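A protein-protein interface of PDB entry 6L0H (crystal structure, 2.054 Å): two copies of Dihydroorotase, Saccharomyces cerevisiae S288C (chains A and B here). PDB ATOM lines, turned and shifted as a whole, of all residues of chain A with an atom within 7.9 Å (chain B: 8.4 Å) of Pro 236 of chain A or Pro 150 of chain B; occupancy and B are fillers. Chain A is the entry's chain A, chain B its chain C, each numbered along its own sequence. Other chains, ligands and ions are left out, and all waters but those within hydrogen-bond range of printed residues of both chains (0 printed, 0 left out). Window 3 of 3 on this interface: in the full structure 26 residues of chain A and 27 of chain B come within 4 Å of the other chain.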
ATOM      1  N   GLU A 184     -14.571   7.265  23.118  1.00  0.00           N
ATOM      2  CA  GLU A 184     -13.184   6.886  23.390  1.00  0.00           C
ATOM      3  C   GLU A 184     -12.668   7.535  24.670  1.00  0.00           C
ATOM      4  O   GLU A 184     -11.954   6.896  25.456  1.00  0.00           O
ATOM      5  CB  GLU A 184     -12.294   7.277  22.197  1.00  0.00           C
ATOM      6  CG  GLU A 184     -10.776   7.018  22.381  1.00  0.00           C
ATOM      7  CD  GLU A 184      -9.978   7.158  21.057  1.00  0.00           C
ATOM      8  OE1 GLU A 184     -10.294   8.071  20.239  1.00  0.00           O
ATOM      9  OE2 GLU A 184      -9.061   6.333  20.830  1.00  0.00           O
ATOM     10  N   LEU A 216     -23.330   1.081  15.713  1.00  0.00           N
ATOM     11  CA  LEU A 216     -23.866   2.342  15.218  1.00  0.00           C
ATOM     12  C   LEU A 216     -22.848   3.457  15.298  1.00  0.00           C
ATOM     13  O   LEU A 216     -21.970   3.490  16.173  1.00  0.00           O
ATOM     14  CB  LEU A 216     -25.104   2.791  15.996  1.00  0.00           C
ATOM     15  CG  LEU A 216     -26.294   1.852  15.952  1.00  0.00           C
ATOM     16  CD1 LEU A 216     -27.421   2.411  16.817  1.00  0.00           C
ATOM     17  CD2 LEU A 216     -26.750   1.583  14.512  1.00  0.00           C
ATOM     18  N   THR A 217     -23.032   4.395  14.384  1.00  0.00           N
ATOM     19  CA  THR A 217     -22.310   5.637  14.255  1.00  0.00           C
ATOM     20  C   THR A 217     -23.353   6.735  14.010  1.00  0.00           C
ATOM     21  O   THR A 217     -24.535   6.448  13.758  1.00  0.00           O
ATOM     22  CB  THR A 217     -21.280   5.455  13.119  1.00  0.00           C
ATOM     23  OG1 THR A 217     -19.977   5.279  13.682  1.00  0.00           O
ATOM     24  CG2 THR A 217     -21.300   6.546  12.121  1.00  0.00           C
ATOM     25  N   ILE A 218     -22.930   8.001  14.116  1.00  0.00           N
ATOM     26  CA  ILE A 218     -23.851   9.120  13.920  1.00  0.00           C
ATOM     27  C   ILE A 218     -24.600   8.998  12.600  1.00  0.00           C
ATOM     28  O   ILE A 218     -25.793   9.317  12.526  1.00  0.00           O
ATOM     29  CB  ILE A 218     -23.116  10.477  14.023  1.00  0.00           C
ATOM     30  CG1 ILE A 218     -24.121  11.617  13.835  1.00  0.00           C
ATOM     31  CG2 ILE A 218     -21.974  10.584  12.996  1.00  0.00           C
ATOM     32  CD1 ILE A 218     -23.610  12.965  14.293  1.00  0.00           C
ATOM     33  N   ASP A 219     -23.932   8.514  11.547  1.00  0.00           N
ATOM     34  CA  ASP A 219     -24.608   8.319  10.266  1.00  0.00           C
ATOM     35  C   ASP A 219     -25.799   7.375  10.360  1.00  0.00           C
ATOM     36  O   ASP A 219     -26.756   7.522   9.596  1.00  0.00           O
ATOM     37  CB  ASP A 219     -23.637   7.807   9.212  1.00  0.00           C
ATOM     38  CG  ASP A 219     -22.919   8.930   8.495  1.00  0.00           C
ATOM     39  OD1 ASP A 219     -22.871  10.040   9.057  1.00  0.00           O
ATOM     40  OD2 ASP A 219     -22.396   8.696   7.384  1.00  0.00           O
ATOM     41  N   ALA A 233     -25.070   7.625  19.583  1.00  0.00           N
ATOM     42  CA  ALA A 233     -23.923   7.028  18.890  1.00  0.00           C
ATOM     43  C   ALA A 233     -23.079   8.109  18.216  1.00  0.00           C
ATOM     44  O   ALA A 233     -23.607   9.019  17.571  1.00  0.00           O
ATOM     45  CB  ALA A 233     -24.381   5.999  17.843  1.00  0.00           C
ATOM     46  N   LYS A 234     -21.764   7.998  18.344  1.00  0.00           N
ATOM     47  CA  LYS A 234     -20.853   9.093  18.019  1.00  0.00           C
ATOM     48  C   LYS A 234     -20.038   8.725  16.780  1.00  0.00           C
ATOM     49  O   LYS A 234     -20.635   8.285  15.792  1.00  0.00           O
ATOM     50  CB  LYS A 234     -20.060   9.445  19.270  1.00  0.00           C
ATOM     51  CG  LYS A 234     -21.003   9.827  20.435  1.00  0.00           C
ATOM     52  CD  LYS A 234     -20.280  10.163  21.716  1.00  0.00           C
ATOM     53  CE  LYS A 234     -21.236  10.812  22.725  1.00  0.00           C
ATOM     54  NZ  LYS A 234     -22.448   9.976  23.029  1.00  0.00           N
ATOM     55  N   LEU A 235     -18.733   8.906  16.768  1.00  0.00           N
ATOM     56  CA  LEU A 235     -17.928   8.837  15.553  1.00  0.00           C
ATOM     57  C   LEU A 235     -17.285   7.473  15.361  1.00  0.00           C
ATOM     58  O   LEU A 235     -17.067   6.728  16.324  1.00  0.00           O
ATOM     59  CB  LEU A 235     -16.822   9.889  15.616  1.00  0.00           C
ATOM     60  CG  LEU A 235     -17.323  11.324  15.709  1.00  0.00           C
ATOM     61  CD1 LEU A 235     -16.166  12.260  15.397  1.00  0.00           C
ATOM     62  CD2 LEU A 235     -18.485  11.548  14.746  1.00  0.00           C
ATOM     63  N   PRO A 236     -16.867   7.165  14.127  1.00  0.00           N
ATOM     64  CA  PRO A 236     -16.156   5.899  13.897  1.00  0.00           C
ATOM     65  C   PRO A 236     -15.040   5.629  14.873  1.00  0.00           C
ATOM     66  O   PRO A 236     -14.907   4.474  15.299  1.00  0.00           O
ATOM     67  CB  PRO A 236     -15.616   6.061  12.463  1.00  0.00           C
ATOM     68  CG  PRO A 236     -16.626   6.933  11.797  1.00  0.00           C
ATOM     69  CD  PRO A 236     -17.111   7.888  12.854  1.00  0.00           C
ATOM     70  N   ASN A 237     -14.221   6.624  15.260  1.00  0.00           N
ATOM     71  CA  ASN A 237     -13.133   6.227  16.142  1.00  0.00           C
ATOM     72  C   ASN A 237     -13.707   5.866  17.527  1.00  0.00           C
ATOM     73  O   ASN A 237     -13.086   5.113  18.286  1.00  0.00           O
ATOM     74  CB  ASN A 237     -12.086   7.301  16.354  1.00  0.00           C
ATOM     75  CG  ASN A 237     -10.815   6.758  17.067  1.00  0.00           C
ATOM     76  OD1 ASN A 237     -10.819   5.830  17.914  1.00  0.00           O
ATOM     77  ND2 ASN A 237      -9.715   7.465  16.811  1.00  0.00           N
ATOM     78  N   ASP A 238     -14.827   6.483  17.919  1.00  0.00           N
ATOM     79  CA  ASP A 238     -15.451   6.094  19.186  1.00  0.00           C
ATOM     80  C   ASP A 238     -15.938   4.652  19.106  1.00  0.00           C
ATOM     81  O   ASP A 238     -15.653   3.846  20.002  1.00  0.00           O
ATOM     82  CB  ASP A 238     -16.590   7.039  19.568  1.00  0.00           C
ATOM     83  CG  ASP A 238     -16.135   8.478  19.810  1.00  0.00           C
ATOM     84  OD1 ASP A 238     -15.317   8.718  20.731  1.00  0.00           O
ATOM     85  OD2 ASP A 238     -16.577   9.381  19.064  1.00  0.00           O
ATOM     86  N   LYS A 239     -16.672   4.309  18.036  1.00  0.00           N
ATOM     87  CA  LYS A 239     -17.106   2.931  17.845  1.00  0.00           C
ATOM     88  C   LYS A 239     -15.937   1.953  17.952  1.00  0.00           C
ATOM     89  O   LYS A 239     -16.060   0.914  18.603  1.00  0.00           O
ATOM     90  CB  LYS A 239     -17.798   2.752  16.497  1.00  0.00           C
ATOM     91  CG  LYS A 239     -18.304   1.299  16.290  1.00  0.00           C
ATOM     92  CD  LYS A 239     -19.183   1.131  15.042  1.00  0.00           C
ATOM     93  CE  LYS A 239     -18.386   0.631  13.849  1.00  0.00           C
ATOM     94  NZ  LYS A 239     -19.299   0.366  12.697  1.00  0.00           N
ATOM     95  N   LYS A 240     -14.781   2.291  17.360  1.00  0.00           N
ATOM     96  CA  LYS A 240     -13.641   1.378  17.382  1.00  0.00           C
ATOM     97  C   LYS A 240     -13.150   1.156  18.796  1.00  0.00           C
ATOM     98  O   LYS A 240     -12.937   0.016  19.211  1.00  0.00           O
ATOM     99  CB  LYS A 240     -12.494   1.928  16.516  1.00  0.00           C
ATOM    100  CG  LYS A 240     -11.228   1.041  16.495  1.00  0.00           C
ATOM    101  CD  LYS A 240      -9.976   1.787  15.962  1.00  0.00           C
ATOM    102  CE  LYS A 240      -8.807   0.851  15.659  1.00  0.00           C
ATOM    103  NZ  LYS A 240      -7.845   0.581  16.803  1.00  0.00           N
ATOM    104  N   ALA A 241     -13.047   2.230  19.584  1.00  0.00           N
ATOM    105  CA  ALA A 241     -12.627   2.095  20.974  1.00  0.00           C
ATOM    106  C   ALA A 241     -13.616   1.260  21.790  1.00  0.00           C
ATOM    107  O   ALA A 241     -13.199   0.493  22.668  1.00  0.00           O
ATOM    108  CB  ALA A 241     -12.421   3.472  21.603  1.00  0.00           C
ATOM    109  N   LEU A 242     -14.925   1.375  21.511  1.00  0.00           N
ATOM    110  CA  LEU A 242     -15.909   0.583  22.269  1.00  0.00           C
ATOM    111  C   LEU A 242     -15.786  -0.898  21.947  1.00  0.00           C
ATOM    112  O   LEU A 242     -15.881  -1.747  22.841  1.00  0.00           O
ATOM    113  CB  LEU A 242     -17.341   1.042  21.980  1.00  0.00           C
ATOM    114  CG  LEU A 242     -17.615   2.527  22.167  1.00  0.00           C
ATOM    115  CD1 LEU A 242     -19.050   2.870  21.763  1.00  0.00           C
ATOM    116  CD2 LEU A 242     -17.349   2.922  23.616  1.00  0.00           C
ATOM    117  N   VAL A 243     -15.590  -1.229  20.668  1.00  0.00           N
ATOM    118  CA  VAL A 243     -15.453  -2.627  20.268  1.00  0.00           C
ATOM    119  C   VAL A 243     -14.196  -3.243  20.883  1.00  0.00           C
ATOM    120  O   VAL A 243     -14.225  -4.365  21.411  1.00  0.00           O
ATOM    121  CB  VAL A 243     -15.454  -2.722  18.734  1.00  0.00           C
ATOM    122  CG1 VAL A 243     -15.223  -4.142  18.297  1.00  0.00           C
ATOM    123  CG2 VAL A 243     -16.774  -2.195  18.180  1.00  0.00           C
ATOM    124  N   PRO B 141     -20.061  12.155  -0.156  1.00  0.00           N
ATOM    125  CA  PRO B 141     -20.838  11.022   0.362  1.00  0.00           C
ATOM    126  C   PRO B 141     -20.053  10.239   1.404  1.00  0.00           C
ATOM    127  O   PRO B 141     -18.822  10.206   1.394  1.00  0.00           O
ATOM    128  CB  PRO B 141     -21.118  10.184  -0.892  1.00  0.00           C
ATOM    129  CG  PRO B 141     -20.968  11.157  -2.040  1.00  0.00           C
ATOM    130  CD  PRO B 141     -19.851  12.054  -1.614  1.00  0.00           C
ATOM    131  N   SER B 142     -20.782   9.627   2.329  1.00  0.00           N
ATOM    132  CA  SER B 142     -20.157   8.954   3.466  1.00  0.00           C
ATOM    133  C   SER B 142     -19.421   7.679   3.041  1.00  0.00           C
ATOM    134  O   SER B 142     -19.822   6.986   2.102  1.00  0.00           O
ATOM    135  CB  SER B 142     -21.215   8.599   4.511  1.00  0.00           C
ATOM    136  OG  SER B 142     -21.725   9.753   5.153  1.00  0.00           O
ATOM    137  N   VAL B 143     -18.328   7.372   3.743  1.00  0.00           N
ATOM    138  CA  VAL B 143     -17.529   6.165   3.492  1.00  0.00           C
ATOM    139  C   VAL B 143     -17.051   5.609   4.834  1.00  0.00           C
ATOM    140  O   VAL B 143     -16.541   6.360   5.671  1.00  0.00           O
ATOM    141  CB  VAL B 143     -16.334   6.392   2.533  1.00  0.00           C
ATOM    142  CG1 VAL B 143     -16.725   7.225   1.318  1.00  0.00           C
ATOM    143  CG2 VAL B 143     -15.145   7.025   3.227  1.00  0.00           C
ATOM    144  N   HIS B 144     -17.280   4.304   5.070  1.00  0.00           N
ATOM    145  CA  HIS B 144     -16.910   3.683   6.337  1.00  0.00           C
ATOM    146  C   HIS B 144     -16.064   2.426   6.132  1.00  0.00           C
ATOM    147  O   HIS B 144     -16.182   1.461   6.905  1.00  0.00           O
ATOM    148  CB  HIS B 144     -18.176   3.325   7.121  1.00  0.00           C
ATOM    149  CG  HIS B 144     -19.047   4.498   7.466  1.00  0.00           C
ATOM    150  ND1 HIS B 144     -18.539   5.726   7.833  1.00  0.00           N
ATOM    151  CD2 HIS B 144     -20.395   4.640   7.448  1.00  0.00           C
ATOM    152  CE1 HIS B 144     -19.536   6.564   8.063  1.00  0.00           C
ATOM    153  NE2 HIS B 144     -20.673   5.932   7.829  1.00  0.00           N
ATOM    154  N   ASP B 145     -15.163   2.439   5.151  1.00  0.00           N
ATOM    155  CA  ASP B 145     -14.592   1.175   4.681  1.00  0.00           C
ATOM    156  C   ASP B 145     -13.106   1.200   4.311  1.00  0.00           C
ATOM    157  O   ASP B 145     -12.293   0.523   4.951  1.00  0.00           O
ATOM    158  CB  ASP B 145     -15.393   0.683   3.468  1.00  0.00           C
ATOM    159  CG  ASP B 145     -15.341   1.636   2.323  1.00  0.00           C
ATOM    160  OD1 ASP B 145     -14.481   1.405   1.446  1.00  0.00           O
ATOM    161  OD2 ASP B 145     -16.104   2.639   2.311  1.00  0.00           O
ATOM    162  N   GLY B 146     -12.767   1.942   3.242  1.00  0.00           N
ATOM    163  CA  GLY B 146     -11.428   2.059   2.732  1.00  0.00           C
ATOM    164  C   GLY B 146     -10.600   2.961   3.590  1.00  0.00           C
ATOM    165  O   GLY B 146     -10.677   4.198   3.491  1.00  0.00           O
ATOM    166  N   ASP B 147      -9.778   2.336   4.438  1.00  0.00           N
ATOM    167  CA  ASP B 147      -9.167   3.073   5.537  1.00  0.00           C
ATOM    168  C   ASP B 147      -8.142   4.063   5.019  1.00  0.00           C
ATOM    169  O   ASP B 147      -6.947   3.998   5.318  1.00  0.00           O
ATOM    170  CB  ASP B 147      -8.612   2.106   6.595  1.00  0.00           C
ATOM    171  CG  ASP B 147      -9.696   1.183   7.150  1.00  0.00           C
ATOM    172  OD1 ASP B 147     -10.884   1.450   6.902  1.00  0.00           O
ATOM    173  OD2 ASP B 147      -9.351   0.204   7.859  1.00  0.00           O
ATOM    174  N   LYS B 148      -8.651   4.932   4.161  1.00  0.00           N
ATOM    175  CA  LYS B 148      -8.499   6.371   4.290  1.00  0.00           C
ATOM    176  C   LYS B 148      -9.584   6.893   5.239  1.00  0.00           C
ATOM    177  O   LYS B 148     -10.546   6.155   5.536  1.00  0.00           O
ATOM    178  CB  LYS B 148      -8.550   6.959   2.881  1.00  0.00           C
ATOM    179  CG  LYS B 148      -8.754   8.405   2.845  1.00  0.00           C
ATOM    180  CD  LYS B 148      -8.360   9.049   1.538  1.00  0.00           C
ATOM    181  CE  LYS B 148      -7.889  10.461   1.895  1.00  0.00           C
ATOM    182  NZ  LYS B 148      -9.026  11.427   1.772  1.00  0.00           N
ATOM    183  N   GLU B 149      -9.470   8.157   5.733  1.00  0.00           N
ATOM    184  CA  GLU B 149     -10.394   8.583   6.769  1.00  0.00           C
ATOM    185  C   GLU B 149     -11.847   8.329   6.414  1.00  0.00           C
ATOM    186  O   GLU B 149     -12.270   8.579   5.258  1.00  0.00           O
ATOM    187  CB  GLU B 149     -10.399  10.083   7.071  1.00  0.00           C
ATOM    188  CG  GLU B 149     -10.481  10.623   8.531  1.00  0.00           C
ATOM    189  CD  GLU B 149      -9.621  10.040   9.653  1.00  0.00           C
ATOM    190  OE1 GLU B 149      -8.594   9.390   9.429  1.00  0.00           O
ATOM    191  OE2 GLU B 149     -10.203   9.899  10.741  1.00  0.00           O
ATOM    192  N   PRO B 150     -12.648   7.876   7.366  1.00  0.00           N
ATOM    193  CA  PRO B 150     -14.087   7.818   7.157  1.00  0.00           C
ATOM    194  C   PRO B 150     -14.659   9.218   7.154  1.00  0.00           C
ATOM    195  O   PRO B 150     -14.144  10.132   7.798  1.00  0.00           O
ATOM    196  CB  PRO B 150     -14.568   6.995   8.369  1.00  0.00           C
ATOM    197  CG  PRO B 150     -13.583   7.300   9.449  1.00  0.00           C
ATOM    198  CD  PRO B 150     -12.263   7.601   8.754  1.00  0.00           C
ATOM    199  N   ILE B 151     -15.683   9.417   6.346  1.00  0.00           N
ATOM    200  CA  ILE B 151     -16.434  10.662   6.366  1.00  0.00           C
ATOM    201  C   ILE B 151     -17.898  10.381   6.712  1.00  0.00           C
ATOM    202  O   ILE B 151     -18.482   9.371   6.296  1.00  0.00           O
ATOM    203  CB  ILE B 151     -16.282  11.469   5.066  1.00  0.00           C
ATOM    204  CG1 ILE B 151     -17.249  11.018   4.016  1.00  0.00           C
ATOM    205  CG2 ILE B 151     -14.865  11.416   4.523  1.00  0.00           C
ATOM    206  CD1 ILE B 151     -17.456  12.100   3.107  1.00  0.00           C
ATOM    207  N   HIS B 152     -18.470  11.258   7.533  1.00  0.00           N
ATOM    208  CA  HIS B 152     -19.822  11.085   8.043  1.00  0.00           C
ATOM    209  C   HIS B 152     -20.540  12.424   7.986  1.00  0.00           C
ATOM    210  O   HIS B 152     -19.986  13.422   7.525  1.00  0.00           O
ATOM    211  CB  HIS B 152     -19.758  10.536   9.460  1.00  0.00           C
ATOM    212  CG  HIS B 152     -18.651  11.139  10.251  1.00  0.00           C
ATOM    213  ND1 HIS B 152     -18.717  12.418  10.748  1.00  0.00           N
ATOM    214  CD2 HIS B 152     -17.420  10.669  10.569  1.00  0.00           C
ATOM    215  CE1 HIS B 152     -17.583  12.706  11.360  1.00  0.00           C
ATOM    216  NE2 HIS B 152     -16.781  11.658  11.273  1.00  0.00           N
ATOM    217  N   VAL B 153     -21.795  12.462   8.448  1.00  0.00           N
ATOM    218  CA  VAL B 153     -22.555  13.698   8.312  1.00  0.00           C
ATOM    219  C   VAL B 153     -21.855  14.862   9.017  1.00  0.00           C
ATOM    220  O   VAL B 153     -22.061  16.018   8.650  1.00  0.00           O
ATOM    221  CB  VAL B 153     -24.007  13.503   8.810  1.00  0.00           C
ATOM    222  CG1 VAL B 153     -24.755  12.505   7.927  1.00  0.00           C
ATOM    223  CG2 VAL B 153     -24.033  13.056  10.259  1.00  0.00           C
ATOM    224  N   LEU B 154     -20.979  14.594   9.983  1.00  0.00           N
ATOM    225  CA  LEU B 154     -20.338  15.699  10.690  1.00  0.00           C
ATOM    226  C   LEU B 154     -19.152  16.295   9.936  1.00  0.00           C
ATOM    227  O   LEU B 154     -18.945  17.513   9.972  1.00  0.00           O
ATOM    228  CB  LEU B 154     -19.864  15.225  12.046  1.00  0.00           C
ATOM    229  CG  LEU B 154     -20.877  15.280  13.168  1.00  0.00           C
ATOM    230  CD1 LEU B 154     -20.094  15.072  14.419  1.00  0.00           C
ATOM    231  CD2 LEU B 154     -21.642  16.607  13.205  1.00  0.00           C
ATOM    232  N   ASN B 155     -18.340  15.475   9.273  1.00  0.00           N
ATOM    233  CA  ASN B 155     -17.189  16.030   8.570  1.00  0.00           C
ATOM    234  C   ASN B 155     -17.326  16.031   7.050  1.00  0.00           C
ATOM    235  O   ASN B 155     -16.370  16.409   6.362  1.00  0.00           O
ATOM    236  CB  ASN B 155     -15.905  15.303   8.990  1.00  0.00           C
ATOM    237  CG  ASN B 155     -15.848  13.855   8.526  1.00  0.00           C
ATOM    238  OD1 ASN B 155     -16.787  13.322   7.904  1.00  0.00           O
ATOM    239  ND2 ASN B 155     -14.744  13.197   8.850  1.00  0.00           N
ATOM    240  N   ALA B 156     -18.485  15.639   6.503  1.00  0.00           N
ATOM    241  CA  ALA B 156     -18.619  15.535   5.047  1.00  0.00           C
ATOM    242  C   ALA B 156     -18.469  16.882   4.348  1.00  0.00           C
ATOM    243  O   ALA B 156     -18.016  16.927   3.202  1.00  0.00           O
ATOM    244  CB  ALA B 156     -19.960  14.912   4.677  1.00  0.00           C
ATOM    245  N   ALA B 159     -14.706  17.613   4.391  1.00  0.00           N
ATOM    246  CA  ALA B 159     -14.060  16.720   3.429  1.00  0.00           C
ATOM    247  C   ALA B 159     -14.269  17.156   1.981  1.00  0.00           C
ATOM    248  O   ALA B 159     -13.548  16.684   1.099  1.00  0.00           O
ATOM    249  CB  ALA B 159     -14.578  15.294   3.598  1.00  0.00           C
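OD2 of Asp 219 of chain A lies within hydrogen-bond range of OG of Ser 142 of chain B (2.6 Å).
NE2 of His 144 of chain B lies within hydrogen-bond range of OD2 of Asp 219 of chain A (3.3 Å).
The side-chain carboxylate (OD1) of Asp 219 of chain A lies within hydrogen-bond range of the backbone NH (N) of Val 153 of chain B (2.7 Å).
The backbone NH of Ile 218 of chain A is in hydrogen-bond range of the backbone carbonyl oxygen of Lys 234 of chain A, 2.9 Å away.
The side-chain carboxylate of Asp 238 of chain A lies within hydrogen-bond range of the backbone NH of Leu 235 of chain A (3.2 Å).
The backbone carbonyl oxygen (O) of Ile 151 of chain B sits close to the side-chain hydroxyl (OG) of Ser 142 of chain B (3.5 Å).
O of Pro 150 of chain B sits at hydrogen-bond distance from ND2 of Asn 155 of chain B, 3.3 Å away.
The backbone NH (N) of Leu 154 of chain B sits close to a ring nitrogen (ND1) of His 152 of chain B.
OD1 of Asn 155 of chain B is in hydrogen-bond range of N of His 152 of chain B, at 2.7 Å.
Among the printed residues, pairs that only touch across the chains: Asp 219 of chain A with His 152 of chain B (3.2 Å), Pro 236 of chain A with His 152 of chain B (3.6 Å), Leu 235 of chain A with His 152 of chain B (3.7 Å), Ile 218 of chain A with Leu 154 of chain B (3.8 Å), Pro 236 of chain A with Pro 150 of chain B (3.8 Å), Ile 218 of chain A with Val 153 of chain B (3.9 Å) and Leu 235 of chain A with Leu 154 of chain B (3.9 Å).
Of chain B, only Pro 150 (3.8 Å) and His 152 (3.6 Å) come within 4 Å of Pro 236 of chain A.
Printed residues of chain A within 4 Å of Val 153 of chain B: Ile 218 (3.9 Å) and Asp 219 (2.7 Å).
Printed residues of chain B within 4 Å of Leu 235 of chain A: His 152 (3.7 Å) and Leu 154 (3.9 Å).
Of the printed residues of chain A, Leu 154 of chain B touches Ile 218 (3.8 Å) and Leu 235 (3.9 Å).
Printed residues of chain A within 4 Å of Ser 142 of chain B: Asp 219.
Asp 145 of chain B touches none of the printed residues of chain A.
Asp 238 of chain A touches none of the printed residues of chain B.
The nearest residue of chain A that does not touch Pro 150 of chain B is Asn 237 of chain A (5.9 Å).
The nearest printed residue of chain B that does not touch Ile 218 of chain A is His 152 of chain B (4.2 Å).
Hydrophobic or aromatic side chains of chain B within 4 Å of the printed part of chain A: His 144, Pro 150, His 152, Val 153 and Leu 154.
Of the 16 printed residues of chain A, 4 touch a printed residue of chain B.
Printed residues of chain A that touch a printed residue of chain B: Ile 218, Asp 219, Leu 235 and Pro 236.
No position is printed for both chains.
Of the 10 pairs that touch across the chains among the printed residues, none has its exchanged pair printed and touching as well.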
